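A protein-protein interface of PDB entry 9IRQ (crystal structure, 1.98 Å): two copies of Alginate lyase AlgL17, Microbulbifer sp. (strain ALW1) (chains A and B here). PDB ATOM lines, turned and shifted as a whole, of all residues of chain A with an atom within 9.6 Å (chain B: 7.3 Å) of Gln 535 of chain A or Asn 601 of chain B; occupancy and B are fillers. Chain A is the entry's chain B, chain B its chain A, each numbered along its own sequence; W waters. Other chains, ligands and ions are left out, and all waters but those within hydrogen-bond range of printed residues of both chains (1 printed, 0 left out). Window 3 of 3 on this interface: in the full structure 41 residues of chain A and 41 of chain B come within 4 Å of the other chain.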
ATOM      1  N   GLN A 526       1.406  12.369 -16.126  1.00  0.00           N
ATOM      2  CA  GLN A 526       0.082  12.381 -16.788  1.00  0.00           C
ATOM      3  C   GLN A 526      -0.755  13.553 -16.277  1.00  0.00           C
ATOM      4  O   GLN A 526      -0.936  13.657 -15.077  1.00  0.00           O
ATOM      5  CB  GLN A 526      -0.648  11.076 -16.482  1.00  0.00           C
ATOM      6  CG  GLN A 526      -2.152  11.129 -16.683  1.00  0.00           C
ATOM      7  CD  GLN A 526      -2.506  11.127 -18.146  1.00  0.00           C
ATOM      8  OE1 GLN A 526      -2.038  10.295 -18.915  1.00  0.00           O
ATOM      9  NE2 GLN A 526      -3.351  12.065 -18.533  1.00  0.00           N
ATOM     10  N   LEU A 527      -1.281  14.352 -17.194  1.00  0.00           N
ATOM     11  CA  LEU A 527      -2.140  15.492 -16.805  1.00  0.00           C
ATOM     12  C   LEU A 527      -3.359  14.932 -16.091  1.00  0.00           C
ATOM     13  O   LEU A 527      -3.970  14.020 -16.610  1.00  0.00           O
ATOM     14  CB  LEU A 527      -2.516  16.320 -18.032  1.00  0.00           C
ATOM     15  CG  LEU A 527      -3.356  17.567 -17.769  1.00  0.00           C
ATOM     16  CD1 LEU A 527      -2.676  18.483 -16.769  1.00  0.00           C
ATOM     17  CD2 LEU A 527      -3.627  18.312 -19.060  1.00  0.00           C
ATOM     18  N   VAL A 528      -3.656  15.480 -14.926  1.00  0.00           N
ATOM     19  CA  VAL A 528      -4.748  14.937 -14.083  1.00  0.00           C
ATOM     20  C   VAL A 528      -5.853  15.980 -13.861  1.00  0.00           C
ATOM     21  O   VAL A 528      -7.004  15.582 -13.700  1.00  0.00           O
ATOM     22  CB  VAL A 528      -4.136  14.415 -12.772  1.00  0.00           C
ATOM     23  CG1 VAL A 528      -4.811  14.939 -11.520  1.00  0.00           C
ATOM     24  CG2 VAL A 528      -4.009  12.903 -12.760  1.00  0.00           C
ATOM     25  N   ASP A 529      -5.512  17.264 -13.844  1.00  0.00           N
ATOM     26  CA  ASP A 529      -6.554  18.273 -13.536  1.00  0.00           C
ATOM     27  C   ASP A 529      -6.116  19.686 -13.893  1.00  0.00           C
ATOM     28  O   ASP A 529      -4.903  19.920 -13.962  1.00  0.00           O
ATOM     29  CB  ASP A 529      -6.898  18.315 -12.043  1.00  0.00           C
ATOM     30  CG  ASP A 529      -8.254  18.911 -11.722  1.00  0.00           C
ATOM     31  OD1 ASP A 529      -8.528  19.096 -10.536  1.00  0.00           O
ATOM     32  OD2 ASP A 529      -9.025  19.174 -12.660  1.00  0.00           O
ATOM     33  N   THR A 530      -7.097  20.571 -14.077  1.00  0.00           N
ATOM     34  CA  THR A 530      -6.811  22.002 -14.272  1.00  0.00           C
ATOM     35  C   THR A 530      -7.814  22.867 -13.519  1.00  0.00           C
ATOM     36  O   THR A 530      -8.921  22.392 -13.295  1.00  0.00           O
ATOM     37  CB  THR A 530      -6.740  22.426 -15.742  1.00  0.00           C
ATOM     38  OG1 THR A 530      -7.953  22.057 -16.395  1.00  0.00           O
ATOM     39  CG2 THR A 530      -5.539  21.879 -16.481  1.00  0.00           C
ATOM     40  N   PHE A 532      -9.126  25.431 -14.734  1.00  0.00           N
ATOM     41  CA  PHE A 532      -9.822  26.190 -15.759  1.00  0.00           C
ATOM     42  C   PHE A 532     -10.272  25.230 -16.849  1.00  0.00           C
ATOM     43  O   PHE A 532      -9.851  24.069 -16.897  1.00  0.00           O
ATOM     44  CB  PHE A 532      -8.894  27.246 -16.345  1.00  0.00           C
ATOM     45  CG  PHE A 532      -7.567  26.680 -16.753  1.00  0.00           C
ATOM     46  CD1 PHE A 532      -7.403  26.118 -18.016  1.00  0.00           C
ATOM     47  CD2 PHE A 532      -6.498  26.659 -15.867  1.00  0.00           C
ATOM     48  CE1 PHE A 532      -6.192  25.574 -18.407  1.00  0.00           C
ATOM     49  CE2 PHE A 532      -5.277  26.113 -16.240  1.00  0.00           C
ATOM     50  CZ  PHE A 532      -5.125  25.559 -17.519  1.00  0.00           C
ATOM     51  N   ARG A 533     -11.108  25.733 -17.753  1.00  0.00           N
ATOM     52  CA  ARG A 533     -11.698  24.886 -18.777  1.00  0.00           C
ATOM     53  C   ARG A 533     -10.663  24.535 -19.833  1.00  0.00           C
ATOM     54  O   ARG A 533      -9.965  25.404 -20.367  1.00  0.00           O
ATOM     55  CB  ARG A 533     -12.917  25.567 -19.400  1.00  0.00           C
ATOM     56  CG  ARG A 533     -14.012  25.877 -18.355  1.00  0.00           C
ATOM     57  CD  ARG A 533     -14.696  27.234 -18.584  1.00  0.00           C
ATOM     58  NE  ARG A 533     -13.809  28.210 -19.229  1.00  0.00           N
ATOM     59  CZ  ARG A 533     -12.770  28.813 -18.655  1.00  0.00           C
ATOM     60  NH1 ARG A 533     -12.457  28.572 -17.386  1.00  0.00           N
ATOM     61  NH2 ARG A 533     -12.050  29.673 -19.359  1.00  0.00           N
ATOM     62  N   LEU A 534     -10.558  23.243 -20.115  1.00  0.00           N
ATOM     63  CA  LEU A 534      -9.552  22.737 -21.038  1.00  0.00           C
ATOM     64  C   LEU A 534     -10.124  21.487 -21.684  1.00  0.00           C
ATOM     65  O   LEU A 534     -10.315  20.477 -21.005  1.00  0.00           O
ATOM     66  CB  LEU A 534      -8.248  22.434 -20.304  1.00  0.00           C
ATOM     67  CG  LEU A 534      -7.081  22.083 -21.217  1.00  0.00           C
ATOM     68  CD1 LEU A 534      -6.525  23.354 -21.819  1.00  0.00           C
ATOM     69  CD2 LEU A 534      -5.999  21.309 -20.474  1.00  0.00           C
ATOM     70  N   GLN A 535     -10.422  21.565 -22.975  1.00  0.00           N
ATOM     71  CA  GLN A 535     -10.814  20.403 -23.757  1.00  0.00           C
ATOM     72  C   GLN A 535      -9.883  20.290 -24.957  1.00  0.00           C
ATOM     73  O   GLN A 535      -9.693  21.261 -25.699  1.00  0.00           O
ATOM     74  CB  GLN A 535     -12.273  20.487 -24.208  1.00  0.00           C
ATOM     75  CG  GLN A 535     -13.272  20.468 -23.053  1.00  0.00           C
ATOM     76  CD  GLN A 535     -13.430  19.084 -22.448  1.00  0.00           C
ATOM     77  OE1 GLN A 535     -14.107  18.213 -23.010  1.00  0.00           O
ATOM     78  NE2 GLN A 535     -12.811  18.871 -21.294  1.00  0.00           N
ATOM     79  N   GLY A 536      -9.302  19.103 -25.137  1.00  0.00           N
ATOM     80  CA  GLY A 536      -8.356  18.906 -26.212  1.00  0.00           C
ATOM     81  C   GLY A 536      -9.026  18.791 -27.571  1.00  0.00           C
ATOM     82  O   GLY A 536     -10.166  18.336 -27.694  1.00  0.00           O
ATOM     83  N   PHE A 537      -8.295  19.234 -28.602  1.00  0.00           N
ATOM     84  CA  PHE A 537      -8.712  19.015 -29.982  1.00  0.00           C
ATOM     85  C   PHE A 537      -8.895  17.525 -30.238  1.00  0.00           C
ATOM     86  O   PHE A 537      -8.114  16.679 -29.780  1.00  0.00           O
ATOM     87  CB  PHE A 537      -7.701  19.620 -30.957  1.00  0.00           C
ATOM     88  CG  PHE A 537      -7.500  21.103 -30.763  1.00  0.00           C
ATOM     89  CD1 PHE A 537      -8.539  21.998 -30.999  1.00  0.00           C
ATOM     90  CD2 PHE A 537      -6.288  21.604 -30.324  1.00  0.00           C
ATOM     91  CE1 PHE A 537      -8.362  23.365 -30.807  1.00  0.00           C
ATOM     92  CE2 PHE A 537      -6.102  22.967 -30.132  1.00  0.00           C
ATOM     93  CZ  PHE A 537      -7.139  23.846 -30.367  1.00  0.00           C
ATOM     94  N   THR A 538      -9.955  17.198 -30.957  1.00  0.00           N
ATOM     95  CA  THR A 538     -10.488  15.855 -30.875  1.00  0.00           C
ATOM     96  C   THR A 538     -10.386  15.056 -32.170  1.00  0.00           C
ATOM     97  O   THR A 538     -10.206  13.833 -32.115  1.00  0.00           O
ATOM     98  CB  THR A 538     -11.946  15.932 -30.401  1.00  0.00           C
ATOM     99  OG1 THR A 538     -12.417  14.616 -30.094  1.00  0.00           O
ATOM    100  CG2 THR A 538     -12.835  16.534 -31.470  1.00  0.00           C
ATOM    101  N   ASP A 539     -10.446  15.696 -33.337  1.00  0.00           N
ATOM    102  CA  ASP A 539     -10.412  14.938 -34.582  1.00  0.00           C
ATOM    103  C   ASP A 539      -9.296  15.354 -35.533  1.00  0.00           C
ATOM    104  O   ASP A 539      -9.104  14.693 -36.564  1.00  0.00           O
ATOM    105  CB  ASP A 539     -11.763  15.027 -35.304  1.00  0.00           C
ATOM    106  CG  ASP A 539     -12.354  16.419 -35.259  1.00  0.00           C
ATOM    107  OD1 ASP A 539     -11.625  17.398 -35.543  1.00  0.00           O
ATOM    108  OD2 ASP A 539     -13.561  16.528 -34.944  1.00  0.00           O
ATOM    109  N   SER A 540      -8.551  16.413 -35.223  1.00  0.00           N
ATOM    110  CA  SER A 540      -7.364  16.732 -35.996  1.00  0.00           C
ATOM    111  C   SER A 540      -6.376  17.449 -35.093  1.00  0.00           C
ATOM    112  O   SER A 540      -6.754  18.050 -34.082  1.00  0.00           O
ATOM    113  CB  SER A 540      -7.693  17.583 -37.234  1.00  0.00           C
ATOM    114  OG  SER A 540      -7.613  18.968 -36.944  1.00  0.00           O
ATOM    115  N   LEU A 541      -5.106  17.356 -35.452  1.00  0.00           N
ATOM    116  CA  LEU A 541      -4.033  18.044 -34.750  1.00  0.00           C
ATOM    117  C   LEU A 541      -3.212  18.790 -35.777  1.00  0.00           C
ATOM    118  O   LEU A 541      -2.917  18.246 -36.841  1.00  0.00           O
ATOM    119  CB  LEU A 541      -3.111  17.070 -34.005  1.00  0.00           C
ATOM    120  CG  LEU A 541      -3.583  16.328 -32.751  1.00  0.00           C
ATOM    121  CD1 LEU A 541      -2.466  15.426 -32.201  1.00  0.00           C
ATOM    122  CD2 LEU A 541      -4.090  17.303 -31.685  1.00  0.00           C
ATOM    123  N   LEU A 555      -0.489  21.175 -31.213  1.00  0.00           N
ATOM    124  CA  LEU A 555      -1.317  21.848 -30.215  1.00  0.00           C
ATOM    125  C   LEU A 555      -2.458  20.896 -29.856  1.00  0.00           C
ATOM    126  O   LEU A 555      -3.308  20.590 -30.698  1.00  0.00           O
ATOM    127  CB  LEU A 555      -1.830  23.187 -30.740  1.00  0.00           C
ATOM    128  CG  LEU A 555      -2.642  24.058 -29.761  1.00  0.00           C
ATOM    129  CD1 LEU A 555      -1.868  24.354 -28.469  1.00  0.00           C
ATOM    130  CD2 LEU A 555      -3.091  25.381 -30.420  1.00  0.00           C
ATOM    131  N   LYS A 556      -2.462  20.391 -28.621  1.00  0.00           N
ATOM    132  CA  LYS A 556      -3.522  19.471 -28.232  1.00  0.00           C
ATOM    133  C   LYS A 556      -4.694  20.178 -27.562  1.00  0.00           C
ATOM    134  O   LYS A 556      -5.822  19.676 -27.620  1.00  0.00           O
ATOM    135  CB  LYS A 556      -2.971  18.373 -27.317  1.00  0.00           C
ATOM    136  CG  LYS A 556      -2.112  17.353 -28.097  1.00  0.00           C
ATOM    137  CD  LYS A 556      -1.906  16.057 -27.337  1.00  0.00           C
ATOM    138  CE  LYS A 556      -3.189  15.242 -27.270  1.00  0.00           C
ATOM    139  NZ  LYS A 556      -3.106  13.951 -28.029  1.00  0.00           N
ATOM    140  N   ALA A 557      -4.471  21.334 -26.949  1.00  0.00           N
ATOM    141  CA  ALA A 557      -5.555  22.020 -26.242  1.00  0.00           C
ATOM    142  C   ALA A 557      -5.141  23.456 -25.946  1.00  0.00           C
ATOM    143  O   ALA A 557      -3.955  23.787 -25.897  1.00  0.00           O
ATOM    144  CB  ALA A 557      -5.938  21.307 -24.938  1.00  0.00           C
ATOM    145  N   ARG A 558      -6.144  24.299 -25.733  1.00  0.00           N
ATOM    146  CA  ARG A 558      -5.924  25.719 -25.485  1.00  0.00           C
ATOM    147  C   ARG A 558      -6.842  26.169 -24.361  1.00  0.00           C
ATOM    148  O   ARG A 558      -8.057  25.969 -24.429  1.00  0.00           O
ATOM    149  CB  ARG A 558      -6.186  26.527 -26.763  1.00  0.00           C
ATOM    150  CG  ARG A 558      -6.182  28.032 -26.619  1.00  0.00           C
ATOM    151  CD  ARG A 558      -6.248  28.677 -28.006  1.00  0.00           C
ATOM    152  NE  ARG A 558      -4.932  29.122 -28.464  1.00  0.00           N
ATOM    153  CZ  ARG A 558      -4.550  29.150 -29.740  1.00  0.00           C
ATOM    154  NH1 ARG A 558      -5.382  28.739 -30.689  1.00  0.00           N
ATOM    155  NH2 ARG A 558      -3.333  29.576 -30.066  1.00  0.00           N
ATOM    156  N   GLY A 559      -6.267  26.755 -23.326  1.00  0.00           N
ATOM    157  CA  GLY A 559      -7.050  27.329 -22.251  1.00  0.00           C
ATOM    158  C   GLY A 559      -6.684  28.785 -22.061  1.00  0.00           C
ATOM    159  O   GLY A 559      -5.593  29.226 -22.417  1.00  0.00           O
ATOM    160  N   LYS A 560      -7.631  29.543 -21.517  1.00  0.00           N
ATOM    161  CA  LYS A 560      -7.396  30.940 -21.165  1.00  0.00           C
ATOM    162  C   LYS A 560      -8.024  31.156 -19.798  1.00  0.00           C
ATOM    163  O   LYS A 560      -9.206  31.514 -19.692  1.00  0.00           O
ATOM    164  CB  LYS A 560      -7.964  31.895 -22.212  1.00  0.00           C
ATOM    165  CG  LYS A 560      -7.336  33.281 -22.152  1.00  0.00           C
ATOM    166  CD  LYS A 560      -7.516  34.054 -23.453  1.00  0.00           C
ATOM    167  CE  LYS A 560      -6.636  35.301 -23.472  1.00  0.00           C
ATOM    168  NZ  LYS A 560      -6.768  36.110 -24.731  1.00  0.00           N
ATOM    169  N   THR A 569      -2.141  20.273 -12.782  1.00  0.00           N
ATOM    170  CA  THR A 569      -1.732  19.182 -11.909  1.00  0.00           C
ATOM    171  C   THR A 569      -1.467  17.945 -12.752  1.00  0.00           C
ATOM    172  O   THR A 569      -2.312  17.553 -13.553  1.00  0.00           O
ATOM    173  CB  THR A 569      -2.810  18.870 -10.859  1.00  0.00           C
ATOM    174  OG1 THR A 569      -2.984  20.001  -9.997  1.00  0.00           O
ATOM    175  CG2 THR A 569      -2.409  17.649 -10.031  1.00  0.00           C
ATOM    176  N   LEU A 590      -2.930  29.264 -22.003  1.00  0.00           N
ATOM    177  CA  LEU A 590      -2.139  28.080 -21.688  1.00  0.00           C
ATOM    178  C   LEU A 590      -2.337  27.098 -22.834  1.00  0.00           C
ATOM    179  O   LEU A 590      -3.461  26.653 -23.096  1.00  0.00           O
ATOM    180  CB  LEU A 590      -2.531  27.494 -20.331  1.00  0.00           C
ATOM    181  CG  LEU A 590      -1.745  27.975 -19.094  1.00  0.00           C
ATOM    182  CD1 LEU A 590      -1.543  29.467 -19.109  1.00  0.00           C
ATOM    183  CD2 LEU A 590      -2.492  27.597 -17.831  1.00  0.00           C
ATOM    184  N   PHE A 592      -1.391  23.537 -24.477  1.00  0.00           N
ATOM    185  CA  PHE A 592      -0.924  22.206 -24.116  1.00  0.00           C
ATOM    186  C   PHE A 592      -0.459  21.502 -25.375  1.00  0.00           C
ATOM    187  O   PHE A 592      -1.182  21.476 -26.369  1.00  0.00           O
ATOM    188  CB  PHE A 592      -2.026  21.408 -23.421  1.00  0.00           C
ATOM    189  CG  PHE A 592      -2.362  21.946 -22.059  1.00  0.00           C
ATOM    190  CD1 PHE A 592      -3.004  23.160 -21.924  1.00  0.00           C
ATOM    191  CD2 PHE A 592      -1.978  21.261 -20.915  1.00  0.00           C
ATOM    192  CE1 PHE A 592      -3.277  23.686 -20.657  1.00  0.00           C
ATOM    193  CE2 PHE A 592      -2.253  21.765 -19.660  1.00  0.00           C
ATOM    194  CZ  PHE A 592      -2.907  22.980 -19.530  1.00  0.00           C
ATOM    195  N   PHE B 411      -7.817   5.670 -13.896  1.00  0.00           N
ATOM    196  CA  PHE B 411      -6.740   6.189 -13.051  1.00  0.00           C
ATOM    197  C   PHE B 411      -7.152   5.898 -11.623  1.00  0.00           C
ATOM    198  O   PHE B 411      -7.860   6.681 -10.988  1.00  0.00           O
ATOM    199  CB  PHE B 411      -6.489   7.662 -13.295  1.00  0.00           C
ATOM    200  CG  PHE B 411      -6.017   7.936 -14.675  1.00  0.00           C
ATOM    201  CD1 PHE B 411      -4.675   7.830 -14.991  1.00  0.00           C
ATOM    202  CD2 PHE B 411      -6.919   8.249 -15.672  1.00  0.00           C
ATOM    203  CE1 PHE B 411      -4.233   8.063 -16.284  1.00  0.00           C
ATOM    204  CE2 PHE B 411      -6.491   8.485 -16.957  1.00  0.00           C
ATOM    205  CZ  PHE B 411      -5.146   8.389 -17.268  1.00  0.00           C
ATOM    206  N   LYS B 417      -9.826  12.362 -11.936  1.00  0.00           N
ATOM    207  CA  LYS B 417     -10.125  11.549 -13.113  1.00  0.00           C
ATOM    208  C   LYS B 417     -11.370  10.703 -12.853  1.00  0.00           C
ATOM    209  O   LYS B 417     -11.310   9.480 -12.656  1.00  0.00           O
ATOM    210  CB  LYS B 417      -8.924  10.681 -13.469  1.00  0.00           C
ATOM    211  CG  LYS B 417      -7.725  11.471 -14.024  1.00  0.00           C
ATOM    212  CD  LYS B 417      -8.001  11.941 -15.433  1.00  0.00           C
ATOM    213  CE  LYS B 417      -6.727  12.028 -16.252  1.00  0.00           C
ATOM    214  NZ  LYS B 417      -6.972  12.854 -17.484  1.00  0.00           N
ATOM    215  N   LEU B 423     -13.350   4.997 -17.118  1.00  0.00           N
ATOM    216  CA  LEU B 423     -13.638   6.185 -17.901  1.00  0.00           C
ATOM    217  C   LEU B 423     -14.425   5.817 -19.146  1.00  0.00           C
ATOM    218  O   LEU B 423     -14.586   4.642 -19.487  1.00  0.00           O
ATOM    219  CB  LEU B 423     -12.335   6.887 -18.288  1.00  0.00           C
ATOM    220  CG  LEU B 423     -11.455   7.268 -17.094  1.00  0.00           C
ATOM    221  CD1 LEU B 423     -10.025   7.591 -17.520  1.00  0.00           C
ATOM    222  CD2 LEU B 423     -12.061   8.422 -16.342  1.00  0.00           C
ATOM    223  N   GLN B 424     -14.918   6.845 -19.840  1.00  0.00           N
ATOM    224  CA  GLN B 424     -15.694   6.585 -21.047  1.00  0.00           C
ATOM    225  C   GLN B 424     -14.868   5.811 -22.063  1.00  0.00           C
ATOM    226  O   GLN B 424     -15.372   4.892 -22.720  1.00  0.00           O
ATOM    227  CB  GLN B 424     -16.184   7.899 -21.653  1.00  0.00           C
ATOM    228  CG  GLN B 424     -16.902   7.706 -22.996  1.00  0.00           C
ATOM    229  CD  GLN B 424     -17.756   8.905 -23.401  1.00  0.00           C
ATOM    230  OE1 GLN B 424     -18.429   9.515 -22.564  1.00  0.00           O
ATOM    231  NE2 GLN B 424     -17.731   9.244 -24.696  1.00  0.00           N
ATOM    232  N   GLU B 425     -13.586   6.165 -22.195  1.00  0.00           N
ATOM    233  CA  GLU B 425     -12.697   5.509 -23.143  1.00  0.00           C
ATOM    234  C   GLU B 425     -12.324   4.091 -22.736  1.00  0.00           C
ATOM    235  O   GLU B 425     -11.673   3.395 -23.520  1.00  0.00           O
ATOM    236  CB  GLU B 425     -11.430   6.351 -23.330  1.00  0.00           C
ATOM    237  CG  GLU B 425     -11.685   7.751 -23.909  1.00  0.00           C
ATOM    238  CD  GLU B 425     -12.199   8.781 -22.882  1.00  0.00           C
ATOM    239  OE1 GLU B 425     -12.138   8.534 -21.661  1.00  0.00           O
ATOM    240  OE2 GLU B 425     -12.685   9.851 -23.308  1.00  0.00           O
ATOM    241  N   ASN B 598      -9.893  11.862 -30.402  1.00  0.00           N
ATOM    242  CA  ASN B 598     -11.168  11.901 -29.686  1.00  0.00           C
ATOM    243  C   ASN B 598     -10.977  11.637 -28.194  1.00  0.00           C
ATOM    244  O   ASN B 598     -11.661  10.808 -27.573  1.00  0.00           O
ATOM    245  CB  ASN B 598     -12.152  10.914 -30.309  1.00  0.00           C
ATOM    246  CG  ASN B 598     -12.629  11.383 -31.658  1.00  0.00           C
ATOM    247  OD1 ASN B 598     -13.484  12.257 -31.739  1.00  0.00           O
ATOM    248  ND2 ASN B 598     -12.060  10.824 -32.733  1.00  0.00           N
ATOM    249  N   ASP B 599     -10.026  12.354 -27.610  1.00  0.00           N
ATOM    250  CA  ASP B 599      -9.650  12.162 -26.212  1.00  0.00           C
ATOM    251  C   ASP B 599      -9.618  13.515 -25.517  1.00  0.00           C
ATOM    252  O   ASP B 599      -8.566  13.959 -25.051  1.00  0.00           O
ATOM    253  CB  ASP B 599      -8.302  11.448 -26.114  1.00  0.00           C
ATOM    254  CG  ASP B 599      -7.874  11.210 -24.677  1.00  0.00           C
ATOM    255  OD1 ASP B 599      -8.768  11.137 -23.793  1.00  0.00           O
ATOM    256  OD2 ASP B 599      -6.647  11.120 -24.424  1.00  0.00           O
ATOM    257  N   PRO B 600     -10.772  14.184 -25.393  1.00  0.00           N
ATOM    258  CA  PRO B 600     -10.758  15.592 -24.958  1.00  0.00           C
ATOM    259  C   PRO B 600     -10.331  15.797 -23.510  1.00  0.00           C
ATOM    260  O   PRO B 600      -9.873  16.899 -23.182  1.00  0.00           O
ATOM    261  CB  PRO B 600     -12.204  16.046 -25.187  1.00  0.00           C
ATOM    262  CG  PRO B 600     -13.016  14.789 -25.125  1.00  0.00           C
ATOM    263  CD  PRO B 600     -12.133  13.693 -25.673  1.00  0.00           C
ATOM    264  N   ASN B 601     -10.432  14.781 -22.645  1.00  0.00           N
ATOM    265  CA  ASN B 601     -10.035  14.903 -21.243  1.00  0.00           C
ATOM    266  C   ASN B 601      -8.650  14.314 -20.957  1.00  0.00           C
ATOM    267  O   ASN B 601      -8.321  14.064 -19.789  1.00  0.00           O
ATOM    268  CB  ASN B 601     -11.082  14.249 -20.340  1.00  0.00           C
ATOM    269  CG  ASN B 601     -12.443  14.877 -20.503  1.00  0.00           C
ATOM    270  OD1 ASN B 601     -12.620  16.066 -20.242  1.00  0.00           O
ATOM    271  ND2 ASN B 601     -13.406  14.093 -20.945  1.00  0.00           N
ATOM    272  N   PHE B 602      -7.836  14.095 -21.994  1.00  0.00           N
ATOM    273  CA  PHE B 602      -6.471  13.578 -21.837  1.00  0.00           C
ATOM    274  C   PHE B 602      -6.477  12.265 -21.066  1.00  0.00           C
ATOM    275  O   PHE B 602      -5.724  12.078 -20.111  1.00  0.00           O
ATOM    276  CB  PHE B 602      -5.559  14.602 -21.150  1.00  0.00           C
ATOM    277  CG  PHE B 602      -5.323  15.843 -21.951  1.00  0.00           C
ATOM    278  CD1 PHE B 602      -6.321  16.792 -22.089  1.00  0.00           C
ATOM    279  CD2 PHE B 602      -4.101  16.062 -22.569  1.00  0.00           C
ATOM    280  CE1 PHE B 602      -6.110  17.946 -22.830  1.00  0.00           C
ATOM    281  CE2 PHE B 602      -3.876  17.204 -23.317  1.00  0.00           C
ATOM    282  CZ  PHE B 602      -4.882  18.153 -23.450  1.00  0.00           C
ATOM    283  N   ASN B 603      -7.361  11.355 -21.472  1.00  0.00           N
ATOM    284  CA  ASN B 603      -7.555  10.124 -20.725  1.00  0.00           C
ATOM    285  C   ASN B 603      -6.732   8.954 -21.254  1.00  0.00           C
ATOM    286  O   ASN B 603      -6.622   7.943 -20.562  1.00  0.00           O
ATOM    287  CB  ASN B 603      -9.041   9.738 -20.716  1.00  0.00           C
ATOM    288  CG  ASN B 603      -9.847  10.505 -19.675  1.00  0.00           C
ATOM    289  OD1 ASN B 603      -9.290  11.194 -18.828  1.00  0.00           O
ATOM    290  ND2 ASN B 603     -11.163  10.378 -19.737  1.00  0.00           N
ATOM    291  N   LEU B 604      -6.141   9.057 -22.436  1.00  0.00           N
ATOM    292  CA  LEU B 604      -5.449   7.935 -23.053  1.00  0.00           C
ATOM    293  C   LEU B 604      -3.951   8.198 -23.105  1.00  0.00           C
ATOM    294  O   LEU B 604      -3.534   9.342 -23.278  1.00  0.00           O
ATOM    295  CB  LEU B 604      -5.973   7.699 -24.464  1.00  0.00           C
ATOM    296  CG  LEU B 604      -7.461   7.385 -24.517  1.00  0.00           C
ATOM    297  CD1 LEU B 604      -7.941   7.283 -25.965  1.00  0.00           C
ATOM    298  CD2 LEU B 604      -7.731   6.089 -23.763  1.00  0.00           C
HETATM  299  O   HOH W   1      -8.004  13.870 -28.701  1.00  0.00           O
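The backbone carbonyl oxygen (O) of Leu 527 of chain A sits at hydrogen-bond distance from the side-chain amino group (NZ) of Lys 417 of chain B (3.3 Å).
The backbone NH (N) of Asn 598 of chain B is in hydrogen-bond range of the backbone carbonyl oxygen (O) of Thr 538 of chain A (2.6 Å).
O of Pro 600 of chain B is in hydrogen-bond range of N of Gly 536 of chain A, at 3.0 Å.
The side-chain amide oxygen (OD1) of Asn 601 of chain B sits at hydrogen-bond distance from the side-chain amide nitrogen (NE2) of Gln 535 of chain A (3.0 Å).
The backbone carbonyl oxygen (O) of Phe 602 of chain B sits at hydrogen-bond distance from the side-chain amide nitrogen (NE2) of Gln 526 of chain A, at 2.8 Å.
The backbone carbonyl oxygen (O) of Asn 601 of chain B sits at hydrogen-bond distance from the side-chain amino group (NZ) of Lys 417 of chain B.
The side-chain amino group (NZ) of Lys 417 of chain B sits at hydrogen-bond distance from the backbone carbonyl oxygen (O) of Phe 602 of chain B (3.0 Å).
The side-chain amino group (NZ) of Lys 417 of chain B is in hydrogen-bond range of the side-chain amide oxygen (OD1) of Asn 603 of chain B, 3.2 Å away.
OD1 of Asn 603 of chain B lies close to O of Asn 601 of chain B.
O of Ala 557 of chain A is in hydrogen-bond range of N of Phe 592 of chain A.
Among the printed residues, merely in contact across the chains: Gln 535 of chain A with Pro 600 of chain B, Ala 557 of chain A with Phe 602 of chain B, Gln 526 of chain A with Phe 411 of chain B and Gln 526 of chain A with Lys 417 of chain B.
Printed residues of chain B within 4 Å of Gln 535 of chain A: Pro 600 and Asn 601.
Asn 601 of chain B touches just one residue of chain A: Gln 535 (3.0 Å).
No residue of chain A comes within 4 Å of Asp 599 of chain B.
Pro 600 of chain B touches two residues of chain A.
Of the printed residues of chain A, Asn 598 of chain B touches Thr 538.
Of the printed residues of chain B, Gln 526 of chain A touches Phe 411 (3.7 Å), Lys 417 (3.9 Å) and Phe 602 (2.8 Å).
Printed residues of chain B within 4 Å of Leu 527 of chain A: Lys 417 (3.3 Å).
Printed residues of chain B within 4 Å of Gly 536 of chain A: Pro 600 (3.0 Å).
Of the printed residues of chain B, Ala 557 of chain A touches Phe 602.
Gln 424 of chain B touches none of the printed residues of chain A.
The nearest residue of chain A that does not touch Asn 601 of chain B is Leu 534 of chain A (5.0 Å).
Among the printed residues, 9 pairs touch across the chains.
Among the printed residues, no Asp or Glu carboxylate lies within 4 Å of a Lys or Arg side-chain nitrogen of the other chain.
No position is printed for both chains.
Water W1 lies within hydrogen-bond range of N of Asp 599 of chain B (2.8 Å), O of Phe 537 of chain A (3.0 Å) and N of Asn 598 of chain B (3.2 Å).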
